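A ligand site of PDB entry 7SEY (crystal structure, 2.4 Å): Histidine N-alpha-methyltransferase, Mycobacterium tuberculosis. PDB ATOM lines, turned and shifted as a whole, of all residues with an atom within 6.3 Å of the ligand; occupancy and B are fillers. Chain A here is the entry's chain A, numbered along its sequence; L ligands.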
ATOM      1  N   PRO A  35     -28.769  -5.140   0.401  1.00  0.00           N
ATOM      2  CA  PRO A  35     -29.516  -3.995   0.946  1.00  0.00           C
ATOM      3  C   PRO A  35     -28.982  -2.632   0.506  1.00  0.00           C
ATOM      4  O   PRO A  35     -29.635  -1.614   0.792  1.00  0.00           O
ATOM      5  CB  PRO A  35     -29.377  -4.168   2.464  1.00  0.00           C
ATOM      6  CG  PRO A  35     -28.055  -4.797   2.603  1.00  0.00           C
ATOM      7  CD  PRO A  35     -27.898  -5.741   1.421  1.00  0.00           C
ATOM      8  N   LYS A  36     -27.850  -2.560  -0.208  1.00  0.00           N
ATOM      9  CA  LYS A  36     -27.325  -1.256  -0.610  1.00  0.00           C
ATOM     10  C   LYS A  36     -28.321  -0.512  -1.490  1.00  0.00           C
ATOM     11  O   LYS A  36     -28.354   0.728  -1.493  1.00  0.00           O
ATOM     12  CB  LYS A  36     -25.971  -1.403  -1.312  1.00  0.00           C
ATOM     13  CG  LYS A  36     -25.992  -2.225  -2.610  1.00  0.00           C
ATOM     14  CD  LYS A  36     -24.652  -2.897  -2.915  1.00  0.00           C
ATOM     15  CE  LYS A  36     -23.567  -1.846  -3.074  1.00  0.00           C
ATOM     16  NZ  LYS A  36     -23.645  -1.145  -4.393  1.00  0.00           N
ATOM     17  N   TYR A  39     -31.406   2.555  -0.933  1.00  0.00           N
ATOM     18  CA  TYR A  39     -31.129   3.937  -0.536  1.00  0.00           C
ATOM     19  C   TYR A  39     -31.052   4.903  -1.723  1.00  0.00           C
ATOM     20  O   TYR A  39     -30.129   5.708  -1.844  1.00  0.00           O
ATOM     21  CB  TYR A  39     -29.837   3.983   0.284  1.00  0.00           C
ATOM     22  CG  TYR A  39     -29.904   3.081   1.488  1.00  0.00           C
ATOM     23  CD1 TYR A  39     -29.311   1.819   1.492  1.00  0.00           C
ATOM     24  CD2 TYR A  39     -30.573   3.490   2.644  1.00  0.00           C
ATOM     25  CE1 TYR A  39     -29.384   1.001   2.586  1.00  0.00           C
ATOM     26  CE2 TYR A  39     -30.650   2.668   3.758  1.00  0.00           C
ATOM     27  CZ  TYR A  39     -30.052   1.428   3.725  1.00  0.00           C
ATOM     28  OH  TYR A  39     -30.157   0.636   4.850  1.00  0.00           O
ATOM     29  N   PHE A  47     -35.557   6.056   5.435  1.00  0.00           N
ATOM     30  CA  PHE A  47     -34.683   5.561   6.478  1.00  0.00           C
ATOM     31  C   PHE A  47     -34.547   6.590   7.584  1.00  0.00           C
ATOM     32  O   PHE A  47     -34.617   6.249   8.781  1.00  0.00           O
ATOM     33  CB  PHE A  47     -33.312   5.212   5.903  1.00  0.00           C
ATOM     34  CG  PHE A  47     -32.345   4.757   6.933  1.00  0.00           C
ATOM     35  CD1 PHE A  47     -32.395   3.460   7.429  1.00  0.00           C
ATOM     36  CD2 PHE A  47     -31.402   5.635   7.449  1.00  0.00           C
ATOM     37  CE1 PHE A  47     -31.504   3.032   8.396  1.00  0.00           C
ATOM     38  CE2 PHE A  47     -30.519   5.213   8.416  1.00  0.00           C
ATOM     39  CZ  PHE A  47     -30.572   3.910   8.899  1.00  0.00           C
ATOM     40  N   TYR A  56     -37.289   1.899  16.535  1.00  0.00           N
ATOM     41  CA  TYR A  56     -35.934   1.729  15.964  1.00  0.00           C
ATOM     42  C   TYR A  56     -34.924   2.359  16.911  1.00  0.00           C
ATOM     43  O   TYR A  56     -34.533   3.521  16.774  1.00  0.00           O
ATOM     44  CB  TYR A  56     -35.821   2.311  14.556  1.00  0.00           C
ATOM     45  CG  TYR A  56     -34.600   1.784  13.817  1.00  0.00           C
ATOM     46  CD1 TYR A  56     -34.541   0.448  13.398  1.00  0.00           C
ATOM     47  CD2 TYR A  56     -33.487   2.583  13.580  1.00  0.00           C
ATOM     48  CE1 TYR A  56     -33.424  -0.061  12.745  1.00  0.00           C
ATOM     49  CE2 TYR A  56     -32.362   2.084  12.920  1.00  0.00           C
ATOM     50  CZ  TYR A  56     -32.340   0.765  12.496  1.00  0.00           C
ATOM     51  OH  TYR A  56     -31.242   0.246  11.838  1.00  0.00           O
ATOM     52  N   LEU A  85     -16.333   5.283   6.954  1.00  0.00           N
ATOM     53  CA  LEU A  85     -16.879   4.365   5.940  1.00  0.00           C
ATOM     54  C   LEU A  85     -18.382   4.604   5.815  1.00  0.00           C
ATOM     55  O   LEU A  85     -19.226   3.793   6.213  1.00  0.00           O
ATOM     56  CB  LEU A  85     -16.553   2.926   6.319  1.00  0.00           C
ATOM     57  CG  LEU A  85     -15.077   2.737   6.711  1.00  0.00           C
ATOM     58  CD1 LEU A  85     -14.819   1.314   7.183  1.00  0.00           C
ATOM     59  CD2 LEU A  85     -14.162   3.121   5.547  1.00  0.00           C
ATOM     60  N   GLY A  86     -18.718   5.750   5.235  1.00  0.00           N
ATOM     61  CA  GLY A  86     -20.091   6.197   5.130  1.00  0.00           C
ATOM     62  C   GLY A  86     -20.116   7.608   4.580  1.00  0.00           C
ATOM     63  O   GLY A  86     -19.100   8.129   4.137  1.00  0.00           O
ATOM     64  N   SER A  87     -21.301   8.218   4.644  1.00  0.00           N
ATOM     65  CA  SER A  87     -21.535   9.492   3.968  1.00  0.00           C
ATOM     66  C   SER A  87     -20.968  10.701   4.714  1.00  0.00           C
ATOM     67  O   SER A  87     -20.612  11.697   4.084  1.00  0.00           O
ATOM     68  CB  SER A  87     -23.030   9.687   3.772  1.00  0.00           C
ATOM     69  OG  SER A  87     -23.696   9.607   5.022  1.00  0.00           O
ATOM     70  N   PHE A 112     -15.695   8.269   3.049  1.00  0.00           N
ATOM     71  CA  PHE A 112     -15.502   7.203   2.058  1.00  0.00           C
ATOM     72  C   PHE A 112     -16.851   6.584   1.750  1.00  0.00           C
ATOM     73  O   PHE A 112     -17.415   5.860   2.582  1.00  0.00           O
ATOM     74  CB  PHE A 112     -14.536   6.160   2.585  1.00  0.00           C
ATOM     75  CG  PHE A 112     -14.218   5.095   1.590  1.00  0.00           C
ATOM     76  CD1 PHE A 112     -15.105   4.062   1.345  1.00  0.00           C
ATOM     77  CD2 PHE A 112     -13.012   5.134   0.886  1.00  0.00           C
ATOM     78  CE1 PHE A 112     -14.813   3.067   0.422  1.00  0.00           C
ATOM     79  CE2 PHE A 112     -12.704   4.142  -0.044  1.00  0.00           C
ATOM     80  CZ  PHE A 112     -13.601   3.114  -0.279  1.00  0.00           C
ATOM     81  N   ASP A 113     -17.361   6.834   0.545  1.00  0.00           N
ATOM     82  CA  ASP A 113     -18.643   6.313   0.116  1.00  0.00           C
ATOM     83  C   ASP A 113     -18.648   6.180  -1.397  1.00  0.00           C
ATOM     84  O   ASP A 113     -17.691   6.554  -2.094  1.00  0.00           O
ATOM     85  CB  ASP A 113     -19.794   7.198   0.591  1.00  0.00           C
ATOM     86  CG  ASP A 113     -21.009   6.393   1.004  1.00  0.00           C
ATOM     87  OD1 ASP A 113     -21.098   5.209   0.575  1.00  0.00           O
ATOM     88  OD2 ASP A 113     -21.873   6.914   1.756  1.00  0.00           O
ATOM     89  N   VAL A 114     -19.751   5.640  -1.917  1.00  0.00           N
ATOM     90  CA  VAL A 114     -19.896   5.328  -3.332  1.00  0.00           C
ATOM     91  C   VAL A 114     -20.755   6.366  -4.057  1.00  0.00           C
ATOM     92  O   VAL A 114     -21.214   6.091  -5.165  1.00  0.00           O
ATOM     93  CB  VAL A 114     -20.478   3.920  -3.549  1.00  0.00           C
ATOM     94  CG1 VAL A 114     -19.523   2.860  -3.059  1.00  0.00           C
ATOM     95  CG2 VAL A 114     -21.825   3.792  -2.852  1.00  0.00           C
ATOM     96  N   PHE A 142     -15.589  -0.929  -1.112  1.00  0.00           N
ATOM     97  CA  PHE A 142     -14.729  -1.579  -0.115  1.00  0.00           C
ATOM     98  C   PHE A 142     -13.797  -2.617  -0.753  1.00  0.00           C
ATOM     99  O   PHE A 142     -12.610  -2.678  -0.417  1.00  0.00           O
ATOM    100  CB  PHE A 142     -15.593  -2.217   0.974  1.00  0.00           C
ATOM    101  CG  PHE A 142     -16.366  -1.219   1.826  1.00  0.00           C
ATOM    102  CD1 PHE A 142     -15.952   0.108   1.927  1.00  0.00           C
ATOM    103  CD2 PHE A 142     -17.499  -1.610   2.533  1.00  0.00           C
ATOM    104  CE1 PHE A 142     -16.655   1.028   2.715  1.00  0.00           C
ATOM    105  CE2 PHE A 142     -18.209  -0.698   3.318  1.00  0.00           C
ATOM    106  CZ  PHE A 142     -17.788   0.620   3.397  1.00  0.00           C
ATOM    107  N   PHE A 159     -16.964   2.832  11.425  1.00  0.00           N
ATOM    108  CA  PHE A 159     -18.002   2.097  10.711  1.00  0.00           C
ATOM    109  C   PHE A 159     -19.158   1.844  11.683  1.00  0.00           C
ATOM    110  O   PHE A 159     -19.205   0.796  12.337  1.00  0.00           O
ATOM    111  CB  PHE A 159     -17.461   0.808  10.123  1.00  0.00           C
ATOM    112  CG  PHE A 159     -18.334   0.201   9.053  1.00  0.00           C
ATOM    113  CD1 PHE A 159     -18.981   1.005   8.124  1.00  0.00           C
ATOM    114  CD2 PHE A 159     -18.499  -1.175   8.974  1.00  0.00           C
ATOM    115  CE1 PHE A 159     -19.777   0.457   7.126  1.00  0.00           C
ATOM    116  CE2 PHE A 159     -19.290  -1.733   7.995  1.00  0.00           C
ATOM    117  CZ  PHE A 159     -19.924  -0.911   7.062  1.00  0.00           C
ATOM    118  N   LEU A 160     -20.079   2.790  11.750  1.00  0.00           N
ATOM    119  CA  LEU A 160     -21.136   2.839  12.756  1.00  0.00           C
ATOM    120  C   LEU A 160     -22.442   2.277  12.209  1.00  0.00           C
ATOM    121  O   LEU A 160     -22.547   1.852  11.050  1.00  0.00           O
ATOM    122  CB  LEU A 160     -21.318   4.281  13.234  1.00  0.00           C
ATOM    123  CG  LEU A 160     -20.051   4.911  13.819  1.00  0.00           C
ATOM    124  CD1 LEU A 160     -20.330   6.224  14.521  1.00  0.00           C
ATOM    125  CD2 LEU A 160     -19.360   3.931  14.750  1.00  0.00           C
ATOM    126  N   GLY A 161     -23.455   2.272  13.066  1.00  0.00           N
ATOM    127  CA  GLY A 161     -24.804   1.929  12.640  1.00  0.00           C
ATOM    128  C   GLY A 161     -25.122   0.454  12.643  1.00  0.00           C
ATOM    129  O   GLY A 161     -26.251   0.073  12.267  1.00  0.00           O
ATOM    130  N   SER A 162     -24.180  -0.394  13.072  1.00  0.00           N
ATOM    131  CA  SER A 162     -24.328  -1.836  12.930  1.00  0.00           C
ATOM    132  C   SER A 162     -24.491  -2.224  11.475  1.00  0.00           C
ATOM    133  O   SER A 162     -25.136  -3.224  11.153  1.00  0.00           O
ATOM    134  CB  SER A 162     -25.487  -2.368  13.790  1.00  0.00           C
ATOM    135  OG  SER A 162     -25.469  -3.789  13.856  1.00  0.00           O
ATOM    136  N   THR A 163     -23.901  -1.403  10.575  1.00  0.00           N
ATOM    137  CA  THR A 163     -23.908  -1.683   9.145  1.00  0.00           C
ATOM    138  C   THR A 163     -23.122  -2.959   8.842  1.00  0.00           C
ATOM    139  O   THR A 163     -23.450  -3.698   7.893  1.00  0.00           O
ATOM    140  CB  THR A 163     -23.311  -0.510   8.364  1.00  0.00           C
ATOM    141  OG1 THR A 163     -24.024   0.696   8.678  1.00  0.00           O
ATOM    142  CG2 THR A 163     -23.410  -0.734   6.863  1.00  0.00           C
ATOM    143  N   ASN A 166     -24.875  -6.265   8.103  1.00  0.00           N
ATOM    144  CA  ASN A 166     -25.339  -6.647   6.772  1.00  0.00           C
ATOM    145  C   ASN A 166     -24.473  -7.708   6.115  1.00  0.00           C
ATOM    146  O   ASN A 166     -24.880  -8.241   5.077  1.00  0.00           O
ATOM    147  CB  ASN A 166     -25.379  -5.449   5.850  1.00  0.00           C
ATOM    148  CG  ASN A 166     -26.512  -4.537   6.146  1.00  0.00           C
ATOM    149  OD1 ASN A 166     -27.520  -4.920   6.725  1.00  0.00           O
ATOM    150  ND2 ASN A 166     -26.389  -3.321   5.691  1.00  0.00           N
ATOM    151  N   TYR A 206     -38.025  -3.734  13.061  1.00  0.00           N
ATOM    152  CA  TYR A 206     -38.009  -3.868  11.614  1.00  0.00           C
ATOM    153  C   TYR A 206     -39.414  -4.147  11.054  1.00  0.00           C
ATOM    154  O   TYR A 206     -39.550  -4.610   9.923  1.00  0.00           O
ATOM    155  CB  TYR A 206     -37.032  -4.965  11.182  1.00  0.00           C
ATOM    156  CG  TYR A 206     -35.562  -4.670  11.467  1.00  0.00           C
ATOM    157  CD1 TYR A 206     -35.043  -4.853  12.751  1.00  0.00           C
ATOM    158  CD2 TYR A 206     -34.694  -4.254  10.447  1.00  0.00           C
ATOM    159  CE1 TYR A 206     -33.709  -4.607  13.017  1.00  0.00           C
ATOM    160  CE2 TYR A 206     -33.346  -4.006  10.716  1.00  0.00           C
ATOM    161  CZ  TYR A 206     -32.861  -4.183  12.016  1.00  0.00           C
ATOM    162  OH  TYR A 206     -31.538  -3.948  12.329  1.00  0.00           O
ATOM    163  N   GLU A 282     -32.507  -8.009   3.091  1.00  0.00           N
ATOM    164  CA  GLU A 282     -31.544  -7.459   4.032  1.00  0.00           C
ATOM    165  C   GLU A 282     -31.323  -8.450   5.153  1.00  0.00           C
ATOM    166  O   GLU A 282     -32.253  -9.123   5.593  1.00  0.00           O
ATOM    167  CB  GLU A 282     -32.013  -6.106   4.618  1.00  0.00           C
ATOM    168  CG  GLU A 282     -31.000  -5.468   5.610  1.00  0.00           C
ATOM    169  CD  GLU A 282     -31.413  -4.064   6.124  1.00  0.00           C
ATOM    170  OE1 GLU A 282     -32.314  -3.952   6.968  1.00  0.00           O
ATOM    171  OE2 GLU A 282     -30.819  -3.072   5.660  1.00  0.00           O
ATOM    172  N   VAL A 283     -30.066  -8.543   5.612  1.00  0.00           N
ATOM    173  CA  VAL A 283     -29.734  -9.244   6.850  1.00  0.00           C
ATOM    174  C   VAL A 283     -29.136  -8.228   7.813  1.00  0.00           C
ATOM    175  O   VAL A 283     -28.217  -7.481   7.438  1.00  0.00           O
ATOM    176  CB  VAL A 283     -28.761 -10.416   6.631  1.00  0.00           C
ATOM    177  CG1 VAL A 283     -29.474 -11.581   5.946  1.00  0.00           C
ATOM    178  CG2 VAL A 283     -27.542  -9.982   5.847  1.00  0.00           C
ATOM    179  N   SER A 284     -29.658  -8.185   9.037  1.00  0.00           N
ATOM    180  CA  SER A 284     -29.003  -7.483  10.143  1.00  0.00           C
ATOM    181  C   SER A 284     -28.637  -8.555  11.162  1.00  0.00           C
ATOM    182  O   SER A 284     -29.485  -8.996  11.931  1.00  0.00           O
ATOM    183  CB  SER A 284     -29.891  -6.403  10.758  1.00  0.00           C
ATOM    184  OG  SER A 284     -30.325  -5.468   9.788  1.00  0.00           O
ATOM    185  N   LYS A 286     -27.222  -9.739  14.599  1.00  0.00           N
ATOM    186  CA  LYS A 286     -27.193  -9.202  15.953  1.00  0.00           C
ATOM    187  C   LYS A 286     -26.063  -9.876  16.731  1.00  0.00           C
ATOM    188  O   LYS A 286     -25.815 -11.075  16.548  1.00  0.00           O
ATOM    189  CB  LYS A 286     -28.522  -9.422  16.655  1.00  0.00           C
ATOM    190  CG  LYS A 286     -29.675  -8.633  16.064  1.00  0.00           C
ATOM    191  CD  LYS A 286     -29.292  -7.194  15.754  1.00  0.00           C
ATOM    192  CE  LYS A 286     -30.378  -6.552  14.906  1.00  0.00           C
ATOM    193  NZ  LYS A 286     -29.967  -5.304  14.216  1.00  0.00           N
HETATM  194  C1  LIG L   1     -22.747   2.741   5.806  1.00  0.00           C
HETATM  195  N1  LIG L   1     -20.738   2.374   2.700  1.00  0.00           N
HETATM  196  C2  LIG L   1     -21.633   2.578   1.715  1.00  0.00           C
HETATM  197  C3  LIG L   1     -26.722   0.908   4.810  1.00  0.00           C
HETATM  198  C4  LIG L   1     -28.035  -0.812   6.386  1.00  0.00           C
HETATM  199  C5  LIG L   1     -29.430  -2.151   8.736  1.00  0.00           C
HETATM  200  C6  LIG L   1     -26.869   2.015   7.168  1.00  0.00           C
HETATM  201  C7  LIG L   1     -24.915   3.234   3.449  1.00  0.00           C
HETATM  202  C8  LIG L   1     -25.709   3.428   2.328  1.00  0.00           C
HETATM  203  C9  LIG L   1     -25.216   3.341   1.036  1.00  0.00           C
HETATM  204  C10 LIG L   1     -23.863   3.064   0.860  1.00  0.00           C
HETATM  205  C11 LIG L   1     -23.010   2.864   1.982  1.00  0.00           C
HETATM  206  C12 LIG L   1     -23.473   2.942   3.279  1.00  0.00           C
HETATM  207  C13 LIG L   1     -22.487   2.710   4.298  1.00  0.00           C
HETATM  208  C14 LIG L   1     -21.165   2.431   3.979  1.00  0.00           C
HETATM  209  C15 LIG L   1     -26.920  -0.518   5.351  1.00  0.00           C
HETATM  210  C16 LIG L   1     -28.444  -0.975   8.886  1.00  0.00           C
HETATM  211  C17 LIG L   1     -26.866   0.769   8.083  1.00  0.00           C
HETATM  212  C18 LIG L   1     -28.330   2.497   7.072  1.00  0.00           C
HETATM  213  N2  LIG L   1     -26.316   1.903   5.789  1.00  0.00           N
HETATM  214  N3  LIG L   1     -27.766  -0.321   7.740  1.00  0.00           N
HETATM  215  N4  LIG L   1     -29.941  -2.520  10.042  1.00  0.00           N
HETATM  216  O1  LIG L   1     -27.104   4.171   4.642  1.00  0.00           O
HETATM  217  O2  LIG L   1     -28.238  -0.605   9.992  1.00  0.00           O
HETATM  218  O3  LIG L   1     -25.301   4.400   5.946  1.00  0.00           O
HETATM  219  S1  LIG L   1     -25.889   3.416   5.014  1.00  0.00           S
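O of Val 283 sits close to OD1 of Asn 166, at 2.7 Å. The backbone carbonyl oxygen (O) of Leu 160 lies within hydrogen-bond range of the side-chain hydroxyl (OG1) of Thr 163, at 3.0 Å. The side-chain carboxylate (OD2) of Asp 113 sits at hydrogen-bond distance from the backbone NH (N) of Ser 87 (3.2 Å). The side-chain hydroxyl (OG) of Ser 284 sits at hydrogen-bond distance from the side-chain hydroxyl (OH) of Tyr 206 (3.2 Å). The side-chain amino group (NZ) of Lys 286 sits at hydrogen-bond distance from the side-chain hydroxyl (OH) of Tyr 206 (2.8 Å).
O of Gly 161 lies close to O2 of the ligand (3.1 Å). Merely in contact with the ligand: Asn 166 (2.9 Å), Thr 163 (2.9 Å), Asp 113 (2.9 Å), Tyr 39 (3.0 Å), Phe 47 (3.2 Å), Leu 85 (3.3 Å), Glu 282 (3.5 Å), Phe 142 (3.5 Å), Tyr 56 (3.5 Å) and Phe 159 (3.97 Å). 13 residues have an atom within 4 Å of the ligand: Tyr 39, Phe 47, Tyr 56, Leu 85, Asp 113, Phe 142, Phe 159, Gly 161, Thr 163, Asn 166, Tyr 206, Glu 282 and Ser 284.
A nitrogen (N4) of the ligand is in hydrogen-bond range of the side-chain hydroxyl of Ser 284, at 3.0 Å. N4 of the ligand lies within hydrogen-bond range of OH of Tyr 206 (3.1 Å).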
